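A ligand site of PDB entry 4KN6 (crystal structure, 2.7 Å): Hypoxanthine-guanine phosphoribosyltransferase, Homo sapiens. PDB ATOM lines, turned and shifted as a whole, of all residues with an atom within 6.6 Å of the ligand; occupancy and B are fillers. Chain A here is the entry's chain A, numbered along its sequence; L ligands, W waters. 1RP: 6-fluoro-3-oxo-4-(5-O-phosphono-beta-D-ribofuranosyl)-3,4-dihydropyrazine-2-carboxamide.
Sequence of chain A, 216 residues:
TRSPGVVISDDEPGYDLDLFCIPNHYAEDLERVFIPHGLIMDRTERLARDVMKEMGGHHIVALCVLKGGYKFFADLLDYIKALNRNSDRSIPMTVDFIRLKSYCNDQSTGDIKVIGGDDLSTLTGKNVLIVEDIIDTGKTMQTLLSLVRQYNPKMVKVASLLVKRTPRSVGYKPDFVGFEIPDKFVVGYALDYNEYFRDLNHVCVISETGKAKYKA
The backbone NH (N) of Gly 138 sits at hydrogen-bond distance from an oxygen (OAH) of the ligand (2.8 Å).
OG1 of Thr 140 is in hydrogen-bond range of OAG of the ligand, at 2.9 Å.
O2' of the ligand sits at hydrogen-bond distance from NZ of Lys 67 (2.7 Å).
N of Thr 137 sits at hydrogen-bond distance from OAC of the ligand (2.9 Å).
The backbone NH (N) of Asp 136 sits at hydrogen-bond distance from an oxygen (OAH) of the ligand.
An oxygen (O2') of the ligand is in hydrogen-bond range of the side-chain carboxylate (OD1) of Asp 133, at 3.4 Å.
O of Val 186 lies within hydrogen-bond range of NAA of the ligand, 3.5 Å away.
OAB of the ligand lies within hydrogen-bond range of NZ of Lys 164, at 2.7 Å.
An oxygen (OAG) of the ligand sits close to the backbone NH (N) of Thr 140.
OG1 of Thr 137 lies within hydrogen-bond range of OAC of the ligand (2.5 Å).
The backbone NH (N) of Lys 164 sits at hydrogen-bond distance from the backbone carbonyl oxygen (O) of Ile 135, at 3.1 Å.
NZ of Lys 67 is in salt-bridge range of OD1 of Asp 133, at 3.0 Å.
NZ of Lys 164 lies within salt-bridge range of OD2 of Asp 136, at 2.8 Å.
The side-chain carboxylate (OD1) of Asp 136 lies within salt-bridge range of the guanidinium group (NH1) of Arg 168 (2.8 Å).
OE2 of Glu 132 lies within salt-bridge range of NZ of Lys 67 (2.9 Å).
The backbone carbonyl oxygen (O) of Lys 184 lies within hydrogen-bond range of the side-chain amino group (NZ) of Lys 164.
FAI of the ligand lies close to O of Asp 192 (3.0 Å).
Residues that only touch the ligand: Glu 132 (3.9 Å), Ile 134 (3.7 Å), Ile 135 (3.8 Å), Lys 139 (3.9 Å), Lys 184 (3.95 Å), Phe 185 (3.4 Å) and Leu 191 (3.7 Å).
Hydrophobic or aromatic side chains within 4 Å of the ligand: Ile 134, Phe 185, Val 186 and Leu 191.
Within 4 Å of the ligand: Lys 67, Glu 132, Asp 133, Ile 134, Ile 135, Asp 136, Thr 137, Gly 138, Lys 139, Thr 140, Lys 164, Lys 184, Phe 185, Val 186, Leu 191 and Asp 192.
Along chain A the residues within 4 Å of the ligand span positions 67 to 192.
Water W1 lies within hydrogen-bond range of OE2 of Glu 132, O of Ile 134 and O3' of the ligand.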
ATOM      1  N   VAL A  65     -19.920  -3.803 -17.301  1.00  0.00           N
ATOM      2  CA  VAL A  65     -20.321  -4.203 -15.963  1.00  0.00           C
ATOM      3  C   VAL A  65     -19.498  -5.427 -15.582  1.00  0.00           C
ATOM      4  O   VAL A  65     -19.442  -6.400 -16.336  1.00  0.00           O
ATOM      5  CB  VAL A  65     -21.820  -4.542 -15.880  1.00  0.00           C
ATOM      6  CG1 VAL A  65     -22.174  -5.045 -14.489  1.00  0.00           C
ATOM      7  CG2 VAL A  65     -22.669  -3.332 -16.238  1.00  0.00           C
ATOM      8  N   LYS A  67     -18.616  -8.360 -12.775  1.00  0.00           N
ATOM      9  CA  LYS A  67     -18.874  -9.137 -11.565  1.00  0.00           C
ATOM     10  C   LYS A  67     -17.922 -10.324 -11.501  1.00  0.00           C
ATOM     11  O   LYS A  67     -16.749 -10.157 -11.164  1.00  0.00           O
ATOM     12  CB  LYS A  67     -20.331  -9.610 -11.518  1.00  0.00           C
ATOM     13  CG  LYS A  67     -21.330  -8.508 -11.201  1.00  0.00           C
ATOM     14  CD  LYS A  67     -22.246  -8.211 -12.372  1.00  0.00           C
ATOM     15  CE  LYS A  67     -23.148  -9.394 -12.689  1.00  0.00           C
ATOM     16  NZ  LYS A  67     -24.059  -9.115 -13.820  1.00  0.00           N
ATOM     17  N   LEU A 100     -19.542  -4.392  -9.489  1.00  0.00           N
ATOM     18  CA  LEU A 100     -20.719  -4.477  -8.618  1.00  0.00           C
ATOM     19  C   LEU A 100     -20.711  -5.782  -7.848  1.00  0.00           C
ATOM     20  O   LEU A 100     -20.140  -6.781  -8.293  1.00  0.00           O
ATOM     21  CB  LEU A 100     -21.999  -4.357  -9.452  1.00  0.00           C
ATOM     22  CG  LEU A 100     -23.322  -4.577  -8.705  1.00  0.00           C
ATOM     23  CD1 LEU A 100     -24.425  -3.729  -9.328  1.00  0.00           C
ATOM     24  CD2 LEU A 100     -23.718  -6.046  -8.703  1.00  0.00           C
ATOM     25  N   GLU A 132     -23.891  -5.667 -20.067  1.00  0.00           N
ATOM     26  CA  GLU A 132     -24.256  -6.561 -18.968  1.00  0.00           C
ATOM     27  C   GLU A 132     -24.526  -7.955 -19.514  1.00  0.00           C
ATOM     28  O   GLU A 132     -24.855  -8.119 -20.697  1.00  0.00           O
ATOM     29  CB  GLU A 132     -25.486  -6.022 -18.234  1.00  0.00           C
ATOM     30  CG  GLU A 132     -25.971  -6.886 -17.084  1.00  0.00           C
ATOM     31  CD  GLU A 132     -24.981  -6.964 -15.942  1.00  0.00           C
ATOM     32  OE1 GLU A 132     -23.803  -7.295 -16.193  1.00  0.00           O
ATOM     33  OE2 GLU A 132     -25.387  -6.684 -14.796  1.00  0.00           O
ATOM     34  N   ASP A 133     -24.404  -8.973 -18.661  1.00  0.00           N
ATOM     35  CA  ASP A 133     -24.646 -10.351 -19.092  1.00  0.00           C
ATOM     36  C   ASP A 133     -26.130 -10.701 -19.077  1.00  0.00           C
ATOM     37  O   ASP A 133     -26.653 -11.215 -20.056  1.00  0.00           O
ATOM     38  CB  ASP A 133     -23.829 -11.353 -18.252  1.00  0.00           C
ATOM     39  CG  ASP A 133     -24.002 -11.156 -16.754  1.00  0.00           C
ATOM     40  OD1 ASP A 133     -24.904 -10.387 -16.347  1.00  0.00           O
ATOM     41  OD2 ASP A 133     -23.235 -11.772 -15.981  1.00  0.00           O
ATOM     42  N   ILE A 134     -26.813 -10.410 -17.965  1.00  0.00           N
ATOM     43  CA  ILE A 134     -28.230 -10.737 -17.853  1.00  0.00           C
ATOM     44  C   ILE A 134     -28.983  -9.804 -16.917  1.00  0.00           C
ATOM     45  O   ILE A 134     -28.473  -9.395 -15.871  1.00  0.00           O
ATOM     46  CB  ILE A 134     -28.434 -12.188 -17.373  1.00  0.00           C
ATOM     47  CG1 ILE A 134     -29.930 -12.531 -17.363  1.00  0.00           C
ATOM     48  CG2 ILE A 134     -27.834 -12.383 -15.991  1.00  0.00           C
ATOM     49  CD1 ILE A 134     -30.209 -14.005 -17.194  1.00  0.00           C
ATOM     50  N   ILE A 135     -30.209  -9.467 -17.313  1.00  0.00           N
ATOM     51  CA  ILE A 135     -31.109  -8.662 -16.493  1.00  0.00           C
ATOM     52  C   ILE A 135     -32.257  -9.545 -16.007  1.00  0.00           C
ATOM     53  O   ILE A 135     -32.966 -10.158 -16.822  1.00  0.00           O
ATOM     54  CB  ILE A 135     -31.700  -7.486 -17.291  1.00  0.00           C
ATOM     55  CG1 ILE A 135     -30.709  -6.314 -17.344  1.00  0.00           C
ATOM     56  CG2 ILE A 135     -32.994  -6.997 -16.657  1.00  0.00           C
ATOM     57  CD1 ILE A 135     -29.251  -6.718 -17.274  1.00  0.00           C
ATOM     58  N   ASP A 136     -32.447  -9.610 -14.699  1.00  0.00           N
ATOM     59  CA  ASP A 136     -33.549 -10.392 -14.126  1.00  0.00           C
ATOM     60  C   ASP A 136     -34.685  -9.488 -13.684  1.00  0.00           C
ATOM     61  O   ASP A 136     -35.736  -9.451 -14.316  1.00  0.00           O
ATOM     62  CB  ASP A 136     -33.054 -11.249 -12.969  1.00  0.00           C
ATOM     63  CG  ASP A 136     -34.046 -12.319 -12.566  1.00  0.00           C
ATOM     64  OD1 ASP A 136     -35.270 -12.103 -12.756  1.00  0.00           O
ATOM     65  OD2 ASP A 136     -33.615 -13.378 -12.059  1.00  0.00           O
ATOM     66  N   THR A 137     -34.463  -8.741 -12.594  1.00  0.00           N
ATOM     67  CA  THR A 137     -35.484  -7.827 -12.084  1.00  0.00           C
ATOM     68  C   THR A 137     -35.294  -6.420 -12.668  1.00  0.00           C
ATOM     69  O   THR A 137     -36.262  -5.669 -12.801  1.00  0.00           O
ATOM     70  CB  THR A 137     -35.467  -7.758 -10.550  1.00  0.00           C
ATOM     71  OG1 THR A 137     -34.154  -7.399 -10.095  1.00  0.00           O
ATOM     72  CG2 THR A 137     -35.865  -9.089  -9.949  1.00  0.00           C
ATOM     73  N   GLY A 138     -34.060  -6.068 -12.987  1.00  0.00           N
ATOM     74  CA  GLY A 138     -33.768  -4.782 -13.605  1.00  0.00           C
ATOM     75  C   GLY A 138     -33.142  -3.788 -12.653  1.00  0.00           C
ATOM     76  O   GLY A 138     -32.357  -2.939 -13.063  1.00  0.00           O
ATOM     77  N   LYS A 139     -33.491  -3.888 -11.369  1.00  0.00           N
ATOM     78  CA  LYS A 139     -32.973  -2.970 -10.359  1.00  0.00           C
ATOM     79  C   LYS A 139     -31.479  -2.722 -10.510  1.00  0.00           C
ATOM     80  O   LYS A 139     -31.029  -1.573 -10.545  1.00  0.00           O
ATOM     81  CB  LYS A 139     -33.271  -3.505  -8.956  1.00  0.00           C
ATOM     82  N   THR A 140     -30.706  -3.799 -10.607  1.00  0.00           N
ATOM     83  CA  THR A 140     -29.255  -3.699 -10.759  1.00  0.00           C
ATOM     84  C   THR A 140     -28.871  -2.686 -11.822  1.00  0.00           C
ATOM     85  O   THR A 140     -28.075  -1.777 -11.573  1.00  0.00           O
ATOM     86  CB  THR A 140     -28.635  -5.062 -11.127  1.00  0.00           C
ATOM     87  OG1 THR A 140     -28.342  -5.801  -9.933  1.00  0.00           O
ATOM     88  CG2 THR A 140     -27.351  -4.890 -11.926  1.00  0.00           C
ATOM     89  N   MET A 141     -29.434  -2.837 -13.016  1.00  0.00           N
ATOM     90  CA  MET A 141     -29.109  -1.972 -14.142  1.00  0.00           C
ATOM     91  C   MET A 141     -29.738  -0.590 -13.964  1.00  0.00           C
ATOM     92  O   MET A 141     -29.113   0.419 -14.258  1.00  0.00           O
ATOM     93  CB  MET A 141     -29.598  -2.593 -15.454  1.00  0.00           C
ATOM     94  CG  MET A 141     -29.278  -1.757 -16.684  1.00  0.00           C
ATOM     95  SD  MET A 141     -27.527  -1.351 -16.807  1.00  0.00           S
ATOM     96  CE  MET A 141     -26.789  -2.981 -16.770  1.00  0.00           C
ATOM     97  N   LYS A 164     -34.702 -11.578 -18.996  1.00  0.00           N
ATOM     98  CA  LYS A 164     -35.645 -12.594 -18.535  1.00  0.00           C
ATOM     99  C   LYS A 164     -37.062 -12.053 -18.419  1.00  0.00           C
ATOM    100  O   LYS A 164     -37.296 -11.025 -17.782  1.00  0.00           O
ATOM    101  CB  LYS A 164     -35.180 -13.122 -17.174  1.00  0.00           C
ATOM    102  CG  LYS A 164     -35.759 -14.469 -16.800  1.00  0.00           C
ATOM    103  CD  LYS A 164     -35.386 -14.851 -15.375  1.00  0.00           C
ATOM    104  CE  LYS A 164     -33.888 -14.890 -15.170  1.00  0.00           C
ATOM    105  NZ  LYS A 164     -33.570 -15.480 -13.838  1.00  0.00           N
ATOM    106  N   ARG A 168     -41.191 -10.276 -11.721  1.00  0.00           N
ATOM    107  CA  ARG A 168     -40.315  -9.663 -10.730  1.00  0.00           C
ATOM    108  C   ARG A 168     -39.532  -8.502 -11.328  1.00  0.00           C
ATOM    109  O   ARG A 168     -38.813  -7.801 -10.618  1.00  0.00           O
ATOM    110  CB  ARG A 168     -39.345 -10.723 -10.185  1.00  0.00           C
ATOM    111  CG  ARG A 168     -40.039 -11.870  -9.472  1.00  0.00           C
ATOM    112  CD  ARG A 168     -39.160 -13.116  -9.401  1.00  0.00           C
ATOM    113  NE  ARG A 168     -37.904 -12.875  -8.705  1.00  0.00           N
ATOM    114  CZ  ARG A 168     -36.687 -12.975  -9.245  1.00  0.00           C
ATOM    115  NH1 ARG A 168     -36.527 -13.320 -10.517  1.00  0.00           N
ATOM    116  NH2 ARG A 168     -35.618 -12.731  -8.500  1.00  0.00           N
ATOM    117  N   ILE A 181     -35.631 -14.834 -22.436  1.00  0.00           N
ATOM    118  CA  ILE A 181     -35.794 -16.220 -21.981  1.00  0.00           C
ATOM    119  C   ILE A 181     -36.799 -16.353 -20.847  1.00  0.00           C
ATOM    120  O   ILE A 181     -37.094 -15.368 -20.153  1.00  0.00           O
ATOM    121  CB  ILE A 181     -34.442 -16.792 -21.506  1.00  0.00           C
ATOM    122  CG1 ILE A 181     -33.875 -15.937 -20.373  1.00  0.00           C
ATOM    123  CG2 ILE A 181     -33.467 -16.853 -22.668  1.00  0.00           C
ATOM    124  CD1 ILE A 181     -32.588 -16.468 -19.779  1.00  0.00           C
ATOM    125  N   LYS A 184     -36.303 -18.631 -15.608  1.00  0.00           N
ATOM    126  CA  LYS A 184     -35.558 -19.732 -15.031  1.00  0.00           C
ATOM    127  C   LYS A 184     -34.150 -19.245 -14.699  1.00  0.00           C
ATOM    128  O   LYS A 184     -33.646 -18.335 -15.344  1.00  0.00           O
ATOM    129  CB  LYS A 184     -35.470 -20.900 -16.015  1.00  0.00           C
ATOM    130  CG  LYS A 184     -36.772 -21.207 -16.736  1.00  0.00           C
ATOM    131  CD  LYS A 184     -37.798 -21.856 -15.825  1.00  0.00           C
ATOM    132  CE  LYS A 184     -37.431 -23.292 -15.495  1.00  0.00           C
ATOM    133  NZ  LYS A 184     -38.529 -23.987 -14.775  1.00  0.00           N
ATOM    134  N   PHE A 185     -33.536 -19.846 -13.686  1.00  0.00           N
ATOM    135  CA  PHE A 185     -32.150 -19.519 -13.358  1.00  0.00           C
ATOM    136  C   PHE A 185     -31.215 -20.326 -14.239  1.00  0.00           C
ATOM    137  O   PHE A 185     -31.123 -21.547 -14.111  1.00  0.00           O
ATOM    138  CB  PHE A 185     -31.855 -19.801 -11.884  1.00  0.00           C
ATOM    139  CG  PHE A 185     -30.556 -19.230 -11.414  1.00  0.00           C
ATOM    140  CD1 PHE A 185     -29.386 -19.972 -11.502  1.00  0.00           C
ATOM    141  CD2 PHE A 185     -30.486 -17.947 -10.884  1.00  0.00           C
ATOM    142  CE1 PHE A 185     -28.186 -19.448 -11.072  1.00  0.00           C
ATOM    143  CE2 PHE A 185     -29.284 -17.431 -10.448  1.00  0.00           C
ATOM    144  CZ  PHE A 185     -28.136 -18.168 -10.540  1.00  0.00           C
ATOM    145  N   VAL A 186     -30.527 -19.639 -15.154  1.00  0.00           N
ATOM    146  CA  VAL A 186     -29.622 -20.301 -16.071  1.00  0.00           C
ATOM    147  C   VAL A 186     -28.160 -20.073 -15.691  1.00  0.00           C
ATOM    148  O   VAL A 186     -27.837 -19.153 -14.947  1.00  0.00           O
ATOM    149  CB  VAL A 186     -29.838 -19.812 -17.526  1.00  0.00           C
ATOM    150  CG1 VAL A 186     -31.271 -20.085 -17.972  1.00  0.00           C
ATOM    151  CG2 VAL A 186     -29.497 -18.335 -17.673  1.00  0.00           C
ATOM    152  N   VAL A 187     -27.298 -20.931 -16.206  1.00  0.00           N
ATOM    153  CA  VAL A 187     -25.868 -20.819 -16.003  1.00  0.00           C
ATOM    154  C   VAL A 187     -25.165 -21.087 -17.321  1.00  0.00           C
ATOM    155  O   VAL A 187     -25.807 -21.515 -18.277  1.00  0.00           O
ATOM    156  CB  VAL A 187     -25.364 -21.825 -14.945  1.00  0.00           C
ATOM    157  CG1 VAL A 187     -25.957 -21.502 -13.580  1.00  0.00           C
ATOM    158  CG2 VAL A 187     -25.721 -23.248 -15.355  1.00  0.00           C
ATOM    159  N   ALA A 190     -21.276 -17.163 -19.729  1.00  0.00           N
ATOM    160  CA  ALA A 190     -20.675 -16.125 -18.898  1.00  0.00           C
ATOM    161  C   ALA A 190     -21.242 -16.159 -17.475  1.00  0.00           C
ATOM    162  O   ALA A 190     -20.729 -15.468 -16.593  1.00  0.00           O
ATOM    163  CB  ALA A 190     -20.909 -14.769 -19.531  1.00  0.00           C
ATOM    164  N   LEU A 191     -22.284 -16.950 -17.261  1.00  0.00           N
ATOM    165  CA  LEU A 191     -22.952 -17.005 -15.973  1.00  0.00           C
ATOM    166  C   LEU A 191     -22.468 -18.214 -15.175  1.00  0.00           C
ATOM    167  O   LEU A 191     -22.250 -19.292 -15.723  1.00  0.00           O
ATOM    168  CB  LEU A 191     -24.465 -17.091 -16.171  1.00  0.00           C
ATOM    169  CG  LEU A 191     -25.055 -15.989 -17.051  1.00  0.00           C
ATOM    170  CD1 LEU A 191     -26.552 -16.204 -17.238  1.00  0.00           C
ATOM    171  CD2 LEU A 191     -24.777 -14.621 -16.459  1.00  0.00           C
ATOM    172  N   ASP A 192     -22.275 -18.009 -13.872  1.00  0.00           N
ATOM    173  CA  ASP A 192     -21.793 -19.063 -13.003  1.00  0.00           C
ATOM    174  C   ASP A 192     -22.784 -19.323 -11.873  1.00  0.00           C
ATOM    175  O   ASP A 192     -23.860 -18.729 -11.836  1.00  0.00           O
ATOM    176  CB  ASP A 192     -20.432 -18.680 -12.429  1.00  0.00           C
ATOM    177  CG  ASP A 192     -20.508 -17.489 -11.501  1.00  0.00           C
ATOM    178  OD1 ASP A 192     -20.653 -16.358 -12.000  1.00  0.00           O
ATOM    179  OD2 ASP A 192     -20.406 -17.686 -10.268  1.00  0.00           O
ATOM    180  N   TYR A 193     -22.408 -20.220 -10.974  1.00  0.00           N
ATOM    181  CA  TYR A 193     -23.213 -20.476  -9.784  1.00  0.00           C
ATOM    182  C   TYR A 193     -22.281 -20.841  -8.637  1.00  0.00           C
ATOM    183  O   TYR A 193     -21.920 -21.990  -8.464  1.00  0.00           O
ATOM    184  CB  TYR A 193     -24.195 -21.612 -10.036  1.00  0.00           C
ATOM    185  CG  TYR A 193     -25.089 -21.891  -8.854  1.00  0.00           C
ATOM    186  CD1 TYR A 193     -26.108 -21.019  -8.500  1.00  0.00           C
ATOM    187  CD2 TYR A 193     -24.918 -23.042  -8.088  1.00  0.00           C
ATOM    188  CE1 TYR A 193     -26.923 -21.275  -7.424  1.00  0.00           C
ATOM    189  CE2 TYR A 193     -25.731 -23.305  -7.005  1.00  0.00           C
ATOM    190  CZ  TYR A 193     -26.735 -22.414  -6.679  1.00  0.00           C
ATOM    191  OH  TYR A 193     -27.550 -22.670  -5.603  1.00  0.00           O
HETATM  192  OAG 1RP L   1     -30.987  -6.771 -10.601  1.00  0.00           O
HETATM  193  PAX 1RP L   1     -31.253  -8.026 -11.480  1.00  0.00           P
HETATM  194  OAH 1RP L   1     -31.792  -7.624 -12.806  1.00  0.00           O
HETATM  195  OAC 1RP L   1     -32.251  -8.914 -10.788  1.00  0.00           O
HETATM  196  O5' 1RP L   1     -29.932  -8.833 -11.656  1.00  0.00           O
HETATM  197  C5' 1RP L   1     -29.524  -9.652 -10.628  1.00  0.00           C
HETATM  198  C4' 1RP L   1     -28.215 -10.225 -10.744  1.00  0.00           C
HETATM  199  O4' 1RP L   1     -28.294 -11.639 -10.746  1.00  0.00           O
HETATM  200  C3' 1RP L   1     -27.627  -9.839 -12.045  1.00  0.00           C
HETATM  201  O3' 1RP L   1     -26.575  -8.991 -11.838  1.00  0.00           O
HETATM  202  C2' 1RP L   1     -27.174 -11.066 -12.644  1.00  0.00           C
HETATM  203  O2' 1RP L   1     -25.900 -10.911 -13.115  1.00  0.00           O
HETATM  204  C1' 1RP L   1     -27.194 -12.048 -11.528  1.00  0.00           C
HETATM  205  NAW 1RP L   1     -27.353 -13.353 -12.067  1.00  0.00           N
HETATM  206  CAQ 1RP L   1     -28.554 -13.722 -12.527  1.00  0.00           C
HETATM  207  OAD 1RP L   1     -29.635 -12.809 -12.470  1.00  0.00           O
HETATM  208  CAJ 1RP L   1     -26.319 -14.202 -12.111  1.00  0.00           C
HETATM  209  CAP 1RP L   1     -26.481 -15.479 -12.645  1.00  0.00           C
HETATM  210  FAI 1RP L   1     -25.488 -16.330 -12.699  1.00  0.00           F
HETATM  211  NAL 1RP L   1     -27.693 -15.835 -13.103  1.00  0.00           N
HETATM  212  CAR 1RP L   1     -28.726 -15.001 -13.060  1.00  0.00           C
HETATM  213  CAO 1RP L   1     -30.088 -15.439 -13.606  1.00  0.00           C
HETATM  214  OAB 1RP L   1     -31.066 -14.622 -13.651  1.00  0.00           O
HETATM  215  NAA 1RP L   1     -30.246 -16.784 -14.064  1.00  0.00           N
HETATM  216  O   HOH W   1     -27.713  -7.281 -14.453  1.00  0.00           O
